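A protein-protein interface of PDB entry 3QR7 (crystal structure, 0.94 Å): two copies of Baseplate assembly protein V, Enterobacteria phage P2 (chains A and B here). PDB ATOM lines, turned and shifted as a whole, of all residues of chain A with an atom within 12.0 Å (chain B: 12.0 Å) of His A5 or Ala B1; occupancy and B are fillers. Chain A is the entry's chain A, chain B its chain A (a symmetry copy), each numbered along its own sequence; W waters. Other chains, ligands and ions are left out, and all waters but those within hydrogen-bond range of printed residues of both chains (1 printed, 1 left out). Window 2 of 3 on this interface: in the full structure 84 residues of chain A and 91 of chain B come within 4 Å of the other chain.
The backbone carbonyl oxygen (O) of His A5 is in hydrogen-bond range of the backbone NH (N) of Ala B1, 2.7 Å away. O of Ala B1 lies within hydrogen-bond range of N of Arg A7, at 3.0 Å. OD2 of Asp A10 is in hydrogen-bond range of OH of Tyr B16, at 2.6 Å.
NH2 of Arg A7 is in salt-bridge range of OE2 of Glu A15 (2.8 Å). The backbone carbonyl oxygen (O) of Ile A14 is in hydrogen-bond range of the backbone NH (N) of Ile A6, 2.9 Å away. The guanidinium group of Arg A7 lies within hydrogen-bond range of a ring nitrogen (NE2) of His A5 (3.4 Å). The side-chain carboxylate (OE2) of Glu A15 lies within hydrogen-bond range of a ring nitrogen (ND1) of His A5. OD1 of Asp A10 is in hydrogen-bond range of N of Ala A12 (3.0 Å). The backbone carbonyl oxygen (O) of Leu B4 is in hydrogen-bond range of the backbone NH (N) of Tyr B16.
O of Ala B1 touches CA of Ile A6 (3.4 Å). Ala B3 touches Ile A6 (N to CG2, 3.5 Å). Arg A7 touches Asp B2. CE1 of Phe A8 touches CA of Ala B3, 3.7 Å away. Leu B4 touches Phe A8 (N to CE1, 3.8 Å). CB of Pro B18 touches CG of Pro A9, 3.9 Å away. O of Pro B18 touches OD2 of Asp A10 (3.6 Å). Tyr B16 touches Ala A12. Ile A14 touches Leu B4. Tyr B16 touches Ile A14 (CB to CD1, 3.8 Å).
No residue of chain B comes within 4 Å of Ala A3. No residue of chain B comes within 4 Å of Leu A4. Of chain B, only Ala B1 comes within 4 Å of His A5. Of the printed residues of chain B, Phe A8 touches Asp B2, Ala B3, Leu B4 and Tyr B16. Of the printed residues of chain B, Asp A10 touches Tyr B16 and Pro B18. Printed residues of chain B within 4 Å of Ala A12: Tyr B16. No residue of chain B comes within 4 Å of Glu A15. Of the printed residues of chain A, Ala B1 touches His A5 (2.7 Å), Ile A6 (3.4 Å) and Arg A7 (3.0 Å). Of chain A, only Ile A6 and Phe A8 come within 4 Å of Ala B3. Of the printed residues of chain A, Leu B4 touches Ile A6, Phe A8 and Ile A14. The nearest residue of chain A that does not touch Ala B1 is Phe A8 (5.4 Å). The nearest printed residue of chain A that does not touch Pro B18 is Phe A8 (4.3 Å).
Printed residues of chain B that touch a printed residue of chain A: Ala B1, Asp B2, Ala B3, Leu B4, Tyr B16 and Pro B18. Hydrophobic or aromatic side chains of chain B within 4 Å of the printed part of chain A: Leu B4, Tyr B16 and Pro B18. Hydrophobic or aromatic side chains of chain A within 4 Å of the printed part of chain B: Ile A6, Phe A8, Pro A9, Ala A12 and Ile A14.
His A5 touches Ala B1, but with the chains exchanged Ala A1 does not touch His B5 (13.9 Å). Ile A6 touches Ala B1, but with the chains exchanged Ala A1 does not touch Ile B6 (10.5 Å). Ile A6 touches Ala B3, but with the chains exchanged Ala A3 does not touch Ile B6 (10.0 Å). Ile A6 touches Leu B4, but with the chains exchanged Leu A4 does not touch Ile B6 (7.6 Å). Positions printed for both chains: 1, 2, 3, 4, 5, 6, 16 and 18.
Water W1 lies within hydrogen-bond range of O of His A5 (2.9 Å) and O of Ala B1 (3.1 Å).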
ATOM      1  N   ALA A   1     -12.660   6.941   6.545  1.00  0.00           N
ATOM      2  CA  ALA A   1     -12.953   5.908   7.540  1.00  0.00           C
ATOM      3  C   ALA A   1     -14.129   4.985   7.290  1.00  0.00           C
ATOM      4  O   ALA A   1     -14.432   4.633   6.035  1.00  0.00           O
ATOM      5  CB  ALA A   1     -12.999   6.526   8.943  1.00  0.00           C
ATOM      6  N   ASP A   2     -14.674   4.503   8.425  1.00  0.00           N
ATOM      7  CA  ASP A   2     -15.730   3.498   8.451  1.00  0.00           C
ATOM      8  C   ASP A   2     -16.841   3.773   9.434  1.00  0.00           C
ATOM      9  O   ASP A   2     -17.642   2.891   9.622  1.00  0.00           O
ATOM     10  CB  ASP A   2     -15.175   2.094   8.649  1.00  0.00           C
ATOM     11  CG  ASP A   2     -14.659   1.884  10.029  1.00  0.00           C
ATOM     12  OD1 ASP A   2     -14.674   2.845  10.823  1.00  0.00           O
ATOM     13  OD2 ASP A   2     -14.201   0.752  10.322  1.00  0.00           O
ATOM     14  N   ALA A   3     -16.965   4.983   9.992  1.00  0.00           N
ATOM     15  CA  ALA A   3     -18.047   5.322  10.941  1.00  0.00           C
ATOM     16  C   ALA A   3     -18.366   6.819  10.899  1.00  0.00           C
ATOM     17  O   ALA A   3     -17.539   7.648  10.550  1.00  0.00           O
ATOM     18  CB  ALA A   3     -17.725   4.902  12.322  1.00  0.00           C
ATOM     19  N   LEU A   4     -19.589   7.137  11.281  1.00  0.00           N
ATOM     20  CA  LEU A   4     -20.085   8.528  11.359  1.00  0.00           C
ATOM     21  C   LEU A   4     -21.096   8.546  12.519  1.00  0.00           C
ATOM     22  O   LEU A   4     -22.182   7.977  12.403  1.00  0.00           O
ATOM     23  CB  LEU A   4     -20.777   8.969  10.085  1.00  0.00           C
ATOM     24  CG  LEU A   4     -21.354  10.398  10.095  1.00  0.00           C
ATOM     25  CD1 LEU A   4     -20.256  11.452  10.178  1.00  0.00           C
ATOM     26  CD2 LEU A   4     -22.240  10.626   8.877  1.00  0.00           C
ATOM     27  N   HIS A   5     -20.723   9.136  13.643  1.00  0.00           N
ATOM     28  CA  HIS A   5     -21.567   9.081  14.823  1.00  0.00           C
ATOM     29  C   HIS A   5     -21.242  10.281  15.709  1.00  0.00           C
ATOM     30  O   HIS A   5     -20.250  10.258  16.418  1.00  0.00           O
ATOM     31  CB  HIS A   5     -21.330   7.756  15.545  1.00  0.00           C
ATOM     32  CG  HIS A   5     -22.240   7.550  16.687  1.00  0.00           C
ATOM     33  ND1 HIS A   5     -23.325   6.712  16.738  1.00  0.00           N
ATOM     34  CD2 HIS A   5     -22.176   8.181  17.883  1.00  0.00           C
ATOM     35  CE1 HIS A   5     -23.849   6.821  17.957  1.00  0.00           C
ATOM     36  NE2 HIS A   5     -23.171   7.711  18.661  1.00  0.00           N
ATOM     37  N   ILE A   6     -22.048  11.329  15.600  1.00  0.00           N
ATOM     38  CA  ILE A   6     -21.723  12.590  16.229  1.00  0.00           C
ATOM     39  C   ILE A   6     -22.909  13.023  17.101  1.00  0.00           C
ATOM     40  O   ILE A   6     -24.074  12.940  16.688  1.00  0.00           O
ATOM     41  CB  ILE A   6     -21.341  13.683  15.211  1.00  0.00           C
ATOM     42  CG1 ILE A   6     -20.480  13.130  14.054  1.00  0.00           C
ATOM     43  CG2 ILE A   6     -20.653  14.792  15.949  1.00  0.00           C
ATOM     44  CD1 ILE A   6     -20.163  14.151  13.000  1.00  0.00           C
ATOM     45  N   ARG A   7     -22.595  13.459  18.304  1.00  0.00           N
ATOM     46  CA  ARG A   7     -23.525  14.012  19.258  1.00  0.00           C
ATOM     47  C   ARG A   7     -22.984  15.395  19.646  1.00  0.00           C
ATOM     48  O   ARG A   7     -21.881  15.483  20.175  1.00  0.00           O
ATOM     49  CB  ARG A   7     -23.649  13.116  20.513  1.00  0.00           C
ATOM     50  CG  ARG A   7     -24.163  11.738  20.209  1.00  0.00           C
ATOM     51  CD  ARG A   7     -25.534  11.719  19.654  1.00  0.00           C
ATOM     52  NE  ARG A   7     -26.077  10.352  19.537  1.00  0.00           N
ATOM     53  CZ  ARG A   7     -26.048   9.563  18.460  1.00  0.00           C
ATOM     54  NH1 ARG A   7     -25.385   9.908  17.382  1.00  0.00           N
ATOM     55  NH2 ARG A   7     -26.718   8.412  18.458  1.00  0.00           N
ATOM     56  N   PHE A   8     -23.760  16.443  19.436  1.00  0.00           N
ATOM     57  CA  PHE A   8     -23.304  17.808  19.600  1.00  0.00           C
ATOM     58  C   PHE A   8     -23.820  18.421  20.894  1.00  0.00           C
ATOM     59  O   PHE A   8     -24.830  17.985  21.450  1.00  0.00           O
ATOM     60  CB  PHE A   8     -23.796  18.635  18.396  1.00  0.00           C
ATOM     61  CG  PHE A   8     -23.226  18.216  17.094  1.00  0.00           C
ATOM     62  CD1 PHE A   8     -21.989  18.683  16.660  1.00  0.00           C
ATOM     63  CD2 PHE A   8     -23.893  17.325  16.263  1.00  0.00           C
ATOM     64  CE1 PHE A   8     -21.486  18.303  15.403  1.00  0.00           C
ATOM     65  CE2 PHE A   8     -23.390  16.966  15.026  1.00  0.00           C
ATOM     66  CZ  PHE A   8     -22.193  17.445  14.599  1.00  0.00           C
ATOM     67  N   PRO A   9     -23.213  19.541  21.350  1.00  0.00           N
ATOM     68  CA  PRO A   9     -23.651  20.089  22.660  1.00  0.00           C
ATOM     69  C   PRO A   9     -24.987  20.773  22.646  1.00  0.00           C
ATOM     70  O   PRO A   9     -25.511  21.040  23.722  1.00  0.00           O
ATOM     71  CB  PRO A   9     -22.530  21.102  23.016  1.00  0.00           C
ATOM     72  CG  PRO A   9     -21.972  21.446  21.668  1.00  0.00           C
ATOM     73  CD  PRO A   9     -21.949  20.149  20.942  1.00  0.00           C
ATOM     74  N   ASP A  10     -25.560  21.030  21.498  1.00  0.00           N
ATOM     75  CA  ASP A  10     -26.908  21.530  21.393  1.00  0.00           C
ATOM     76  C   ASP A  10     -27.959  20.412  21.391  1.00  0.00           C
ATOM     77  O   ASP A  10     -29.140  20.706  21.260  1.00  0.00           O
ATOM     78  CB  ASP A  10     -27.073  22.424  20.183  1.00  0.00           C
ATOM     79  CG  ASP A  10     -26.890  21.683  18.863  1.00  0.00           C
ATOM     80  OD1 ASP A  10     -26.355  20.559  18.868  1.00  0.00           O
ATOM     81  OD2 ASP A  10     -27.275  22.295  17.826  1.00  0.00           O
ATOM     82  N   GLY A  11     -27.514  19.162  21.486  1.00  0.00           N
ATOM     83  CA  GLY A  11     -28.413  18.023  21.400  1.00  0.00           C
ATOM     84  C   GLY A  11     -28.614  17.481  20.006  1.00  0.00           C
ATOM     85  O   GLY A  11     -29.329  16.475  19.843  1.00  0.00           O
ATOM     86  N   ALA A  12     -28.001  18.069  19.000  1.00  0.00           N
ATOM     87  CA  ALA A  12     -28.142  17.540  17.654  1.00  0.00           C
ATOM     88  C   ALA A  12     -27.408  16.205  17.523  1.00  0.00           C
ATOM     89  O   ALA A  12     -26.427  15.912  18.210  1.00  0.00           O
ATOM     90  CB  ALA A  12     -27.619  18.523  16.620  1.00  0.00           C
ATOM     91  N   VAL A  13     -27.899  15.418  16.569  1.00  0.00           N
ATOM     92  CA  VAL A  13     -27.333  14.138  16.163  1.00  0.00           C
ATOM     93  C   VAL A  13     -27.057  14.213  14.658  1.00  0.00           C
ATOM     94  O   VAL A  13     -27.932  14.589  13.896  1.00  0.00           O
ATOM     95  CB  VAL A  13     -28.358  12.995  16.417  1.00  0.00           C
ATOM     96  CG1 VAL A  13     -27.966  11.715  15.703  1.00  0.00           C
ATOM     97  CG2 VAL A  13     -28.580  12.836  17.888  1.00  0.00           C
ATOM     98  N   ILE A  14     -25.861  13.792  14.249  1.00  0.00           N
ATOM     99  CA  ILE A  14     -25.565  13.493  12.854  1.00  0.00           C
ATOM    100  C   ILE A  14     -24.870  12.131  12.858  1.00  0.00           C
ATOM    101  O   ILE A  14     -23.801  11.991  13.436  1.00  0.00           O
ATOM    102  CB  ILE A  14     -24.703  14.543  12.158  1.00  0.00           C
ATOM    103  CG1 ILE A  14     -25.451  15.874  12.105  1.00  0.00           C
ATOM    104  CG2 ILE A  14     -24.295  14.059  10.772  1.00  0.00           C
ATOM    105  CD1 ILE A  14     -24.651  17.037  11.535  1.00  0.00           C
ATOM    106  N   GLU A  15     -25.483  11.143  12.230  1.00  0.00           N
ATOM    107  CA  GLU A  15     -24.894   9.817  12.282  1.00  0.00           C
ATOM    108  C   GLU A  15     -25.362   8.979  11.090  1.00  0.00           C
ATOM    109  O   GLU A  15     -26.378   9.236  10.475  1.00  0.00           O
ATOM    110  CB  GLU A  15     -25.268   9.088  13.561  1.00  0.00           C
ATOM    111  CG  GLU A  15     -26.717   8.732  13.650  1.00  0.00           C
ATOM    112  CD  GLU A  15     -27.013   7.706  14.688  1.00  0.00           C
ATOM    113  OE1 GLU A  15     -27.869   6.828  14.431  1.00  0.00           O
ATOM    114  OE2 GLU A  15     -26.351   7.720  15.750  1.00  0.00           O
ATOM    115  N   TYR A  16     -24.596   7.918  10.865  1.00  0.00           N
ATOM    116  CA  TYR A  16     -25.043   6.819  10.030  1.00  0.00           C
ATOM    117  C   TYR A  16     -24.976   5.538  10.861  1.00  0.00           C
ATOM    118  O   TYR A  16     -23.991   5.277  11.525  1.00  0.00           O
ATOM    119  CB  TYR A  16     -24.181   6.653   8.776  1.00  0.00           C
ATOM    120  CG  TYR A  16     -24.760   5.625   7.847  1.00  0.00           C
ATOM    121  CD1 TYR A  16     -25.951   5.864   7.205  1.00  0.00           C
ATOM    122  CD2 TYR A  16     -24.148   4.397   7.647  1.00  0.00           C
ATOM    123  CE1 TYR A  16     -26.542   4.939   6.384  1.00  0.00           C
ATOM    124  CE2 TYR A  16     -24.720   3.440   6.811  1.00  0.00           C
ATOM    125  CZ  TYR A  16     -25.916   3.714   6.174  1.00  0.00           C
ATOM    126  OH  TYR A  16     -26.504   2.833   5.327  1.00  0.00           O
ATOM    127  N   GLU A  17     -26.061   4.767  10.802  1.00  0.00           N
ATOM    128  CA  GLU A  17     -26.184   3.519  11.544  1.00  0.00           C
ATOM    129  C   GLU A  17     -26.219   2.359  10.540  1.00  0.00           C
ATOM    130  O   GLU A  17     -27.261   2.099   9.951  1.00  0.00           O
ATOM    131  CB  GLU A  17     -27.447   3.555  12.407  1.00  0.00           C
ATOM    132  CG  GLU A  17     -27.648   2.267  13.201  1.00  0.00           C
ATOM    133  CD  GLU A  17     -26.375   1.836  13.891  1.00  0.00           C
ATOM    134  OE1 GLU A  17     -25.963   2.552  14.837  1.00  0.00           O
ATOM    135  OE2 GLU A  17     -25.748   0.848  13.425  1.00  0.00           O
ATOM    136  N   PRO A  18     -25.105   1.658  10.339  1.00  0.00           N
ATOM    137  CA  PRO A  18     -25.124   0.612   9.316  1.00  0.00           C
ATOM    138  C   PRO A  18     -25.965  -0.599   9.694  1.00  0.00           C
ATOM    139  O   PRO A  18     -26.334  -1.346   8.798  1.00  0.00           O
ATOM    140  CB  PRO A  18     -23.625   0.291   9.104  1.00  0.00           C
ATOM    141  CG  PRO A  18     -23.012   0.649  10.463  1.00  0.00           C
ATOM    142  CD  PRO A  18     -23.778   1.827  10.952  1.00  0.00           C
ATOM    143  N   GLU A  19     -26.295  -0.807  10.964  1.00  0.00           N
ATOM    144  CA  GLU A  19     -27.104  -1.974  11.309  1.00  0.00           C
ATOM    145  C   GLU A  19     -28.476  -1.931  10.654  1.00  0.00           C
ATOM    146  O   GLU A  19     -29.022  -2.969  10.322  1.00  0.00           O
ATOM    147  CB  GLU A  19     -27.268  -2.080  12.816  1.00  0.00           C
ATOM    148  CG  GLU A  19     -26.033  -2.486  13.556  1.00  0.00           C
ATOM    149  CD  GLU A  19     -25.729  -3.944  13.374  1.00  0.00           C
ATOM    150  OE1 GLU A  19     -24.823  -4.196  12.536  1.00  0.00           O
ATOM    151  OE2 GLU A  19     -26.311  -4.780  14.074  1.00  0.00           O
ATOM    152  N   THR A  20     -29.043  -0.718  10.530  1.00  0.00           N
ATOM    153  CA  THR A  20     -30.324  -0.473   9.929  1.00  0.00           C
ATOM    154  C   THR A  20     -30.211   0.344   8.617  1.00  0.00           C
ATOM    155  O   THR A  20     -31.209   0.674   7.996  1.00  0.00           O
ATOM    156  CB  THR A  20     -31.240   0.270  10.882  1.00  0.00           C
ATOM    157  OG1 THR A  20     -30.569   1.487  11.196  1.00  0.00           O
ATOM    158  CG2 THR A  20     -31.545  -0.534  12.133  1.00  0.00           C
ATOM    159  N   SER A  21     -28.984   0.686   8.254  1.00  0.00           N
ATOM    160  CA  SER A  21     -28.677   1.505   7.094  1.00  0.00           C
ATOM    161  C   SER A  21     -29.424   2.839   7.102  1.00  0.00           C
ATOM    162  O   SER A  21     -30.000   3.260   6.100  1.00  0.00           O
ATOM    163  CB  SER A  21     -28.902   0.748   5.784  1.00  0.00           C
ATOM    164  OG  SER A  21     -28.181  -0.486   5.768  1.00  0.00           O
ATOM    165  N   ALA A  22     -29.365   3.509   8.252  1.00  0.00           N
ATOM    166  CA  ALA A  22     -30.125   4.737   8.486  1.00  0.00           C
ATOM    167  C   ALA A  22     -29.198   5.917   8.715  1.00  0.00           C
ATOM    168  O   ALA A  22     -28.378   5.928   9.646  1.00  0.00           O
ATOM    169  CB  ALA A  22     -31.034   4.579   9.704  1.00  0.00           C
ATOM    170  N   LEU A  23     -29.365   6.954   7.888  1.00  0.00           N
ATOM    171  CA  LEU A  23     -28.688   8.245   8.046  1.00  0.00           C
ATOM    172  C   LEU A  23     -29.654   9.166   8.810  1.00  0.00           C
ATOM    173  O   LEU A  23     -30.781   9.363   8.364  1.00  0.00           O
ATOM    174  CB  LEU A  23     -28.376   8.831   6.672  1.00  0.00           C
ATOM    175  CG  LEU A  23     -27.779  10.229   6.638  1.00  0.00           C
ATOM    176  CD1 LEU A  23     -26.497  10.364   7.347  1.00  0.00           C
ATOM    177  CD2 LEU A  23     -27.659  10.702   5.169  1.00  0.00           C
ATOM    178  N   THR A  24     -29.207   9.716   9.936  1.00  0.00           N
ATOM    179  CA  THR A  24     -30.045  10.568  10.763  1.00  0.00           C
ATOM    180  C   THR A  24     -29.353  11.887  11.044  1.00  0.00           C
ATOM    181  O   THR A  24     -28.221  11.925  11.519  1.00  0.00           O
ATOM    182  CB  THR A  24     -30.381   9.865  12.095  1.00  0.00           C
ATOM    183  OG1 THR A  24     -31.046   8.640  11.805  1.00  0.00           O
ATOM    184  CG2 THR A  24     -31.241  10.718  12.981  1.00  0.00           C
ATOM    185  N   VAL A  25     -30.117  12.957  10.812  1.00  0.00           N
ATOM    186  CA  VAL A  25     -29.774  14.302  11.253  1.00  0.00           C
ATOM    187  C   VAL A  25     -30.966  14.751  12.087  1.00  0.00           C
ATOM    188  O   VAL A  25     -32.099  14.763  11.585  1.00  0.00           O
ATOM    189  CB  VAL A  25     -29.537  15.249  10.075  1.00  0.00           C
ATOM    190  CG1 VAL A  25     -29.333  16.681  10.577  1.00  0.00           C
ATOM    191  CG2 VAL A  25     -28.373  14.782   9.231  1.00  0.00           C
ATOM    192  N   SER A  26     -30.764  15.088  13.349  1.00  0.00           N
ATOM    193  CA  SER A  26     -31.887  15.494  14.186  1.00  0.00           C
ATOM    194  C   SER A  26     -31.441  16.573  15.148  1.00  0.00           C
ATOM    195  O   SER A  26     -30.253  16.761  15.418  1.00  0.00           O
ATOM    196  CB  SER A  26     -32.486  14.336  14.961  1.00  0.00           C
ATOM    197  OG  SER A  26     -31.576  13.863  15.916  1.00  0.00           O
ATOM    198  N   ALA B   1     -17.894  11.058  17.552  1.00  0.00           N
ATOM    199  CA  ALA B   1     -17.433  12.292  18.190  1.00  0.00           C
ATOM    200  C   ALA B   1     -18.463  13.349  18.533  1.00  0.00           C
ATOM    201  O   ALA B   1     -19.692  12.973  18.902  1.00  0.00           O
ATOM    202  CB  ALA B   1     -16.250  12.878  17.409  1.00  0.00           C
ATOM    203  N   ASP B   2     -17.954  14.597  18.551  1.00  0.00           N
ATOM    204  CA  ASP B   2     -18.706  15.771  18.978  1.00  0.00           C
ATOM    205  C   ASP B   2     -18.535  16.987  18.101  1.00  0.00           C
ATOM    206  O   ASP B   2     -18.990  18.028  18.506  1.00  0.00           O
ATOM    207  CB  ASP B   2     -18.439  16.119  20.436  1.00  0.00           C
ATOM    208  CG  ASP B   2     -17.070  16.670  20.638  1.00  0.00           C
ATOM    209  OD1 ASP B   2     -16.300  16.728  19.659  1.00  0.00           O
ATOM    210  OD2 ASP B   2     -16.742  17.022  21.798  1.00  0.00           O
ATOM    211  N   ALA B   3     -17.978  16.873  16.889  1.00  0.00           N
ATOM    212  CA  ALA B   3     -17.806  18.020  15.973  1.00  0.00           C
ATOM    213  C   ALA B   3     -17.797  17.561  14.513  1.00  0.00           C
ATOM    214  O   ALA B   3     -17.464  16.431  14.191  1.00  0.00           O
ATOM    215  CB  ALA B   3     -16.584  18.794  16.278  1.00  0.00           C
ATOM    216  N   LEU B   4     -18.163  18.481  13.639  1.00  0.00           N
ATOM    217  CA  LEU B   4     -18.179  18.259  12.177  1.00  0.00           C
ATOM    218  C   LEU B   4     -17.846  19.623  11.545  1.00  0.00           C
ATOM    219  O   LEU B   4     -18.663  20.543  11.593  1.00  0.00           O
ATOM    220  CB  LEU B   4     -19.531  17.792  11.677  1.00  0.00           C
ATOM    221  CG  LEU B   4     -19.642  17.568  10.156  1.00  0.00           C
ATOM    222  CD1 LEU B   4     -18.771  16.408   9.688  1.00  0.00           C
ATOM    223  CD2 LEU B   4     -21.095  17.360   9.751  1.00  0.00           C
ATOM    224  N   HIS B   5     -16.643  19.771  11.015  1.00  0.00           N
ATOM    225  CA  HIS B   5     -16.208  21.063  10.517  1.00  0.00           C
ATOM    226  C   HIS B   5     -15.130  20.839   9.461  1.00  0.00           C
ATOM    227  O   HIS B   5     -13.987  20.589   9.807  1.00  0.00           O
ATOM    228  CB  HIS B   5     -15.698  21.903  11.687  1.00  0.00           C
ATOM    229  CG  HIS B   5     -15.355  23.283  11.300  1.00  0.00           C
ATOM    230  ND1 HIS B   5     -16.079  24.419  11.562  1.00  0.00           N
ATOM    231  CD2 HIS B   5     -14.270  23.667  10.587  1.00  0.00           C
ATOM    232  CE1 HIS B   5     -15.400  25.444  11.052  1.00  0.00           C
ATOM    233  NE2 HIS B   5     -14.306  25.008  10.452  1.00  0.00           N
ATOM    234  N   ILE B   6     -15.528  20.869   8.196  1.00  0.00           N
ATOM    235  CA  ILE B   6     -14.644  20.467   7.123  1.00  0.00           C
ATOM    236  C   ILE B   6     -14.580  21.600   6.090  1.00  0.00           C
ATOM    237  O   ILE B   6     -15.605  22.189   5.718  1.00  0.00           O
ATOM    238  CB  ILE B   6     -15.062  19.133   6.475  1.00  0.00           C
ATOM    239  CG1 ILE B   6     -15.563  18.107   7.516  1.00  0.00           C
ATOM    240  CG2 ILE B   6     -13.903  18.613   5.679  1.00  0.00           C
ATOM    241  CD1 ILE B   6     -16.058  16.827   6.907  1.00  0.00           C
ATOM    242  N   TYR B  16     -21.311  21.312  10.825  1.00  0.00           N
ATOM    243  CA  TYR B  16     -22.405  21.606  11.731  1.00  0.00           C
ATOM    244  C   TYR B  16     -21.901  22.607  12.771  1.00  0.00           C
ATOM    245  O   TYR B  16     -20.835  22.438  13.332  1.00  0.00           O
ATOM    246  CB  TYR B  16     -22.923  20.354  12.444  1.00  0.00           C
ATOM    247  CG  TYR B  16     -24.158  20.652  13.243  1.00  0.00           C
ATOM    248  CD1 TYR B  16     -25.331  20.984  12.608  1.00  0.00           C
ATOM    249  CD2 TYR B  16     -24.146  20.652  14.630  1.00  0.00           C
ATOM    250  CE1 TYR B  16     -26.472  21.308  13.295  1.00  0.00           C
ATOM    251  CE2 TYR B  16     -25.294  20.968  15.356  1.00  0.00           C
ATOM    252  CZ  TYR B  16     -26.460  21.291  14.687  1.00  0.00           C
ATOM    253  OH  TYR B  16     -27.613  21.579  15.340  1.00  0.00           O
ATOM    254  N   PRO B  18     -22.986  24.078  16.235  1.00  0.00           N
ATOM    255  CA  PRO B  18     -23.971  23.946  17.310  1.00  0.00           C
ATOM    256  C   PRO B  18     -24.348  25.269  17.960  1.00  0.00           C
ATOM    257  O   PRO B  18     -25.392  25.320  18.597  1.00  0.00           O
ATOM    258  CB  PRO B  18     -23.309  22.939  18.280  1.00  0.00           C
ATOM    259  CG  PRO B  18     -21.814  23.162  18.025  1.00  0.00           C
ATOM    260  CD  PRO B  18     -21.694  23.459  16.572  1.00  0.00           C
HETATM  261  O   HOH W   1     -20.824  10.159  19.294  1.00  0.00           O
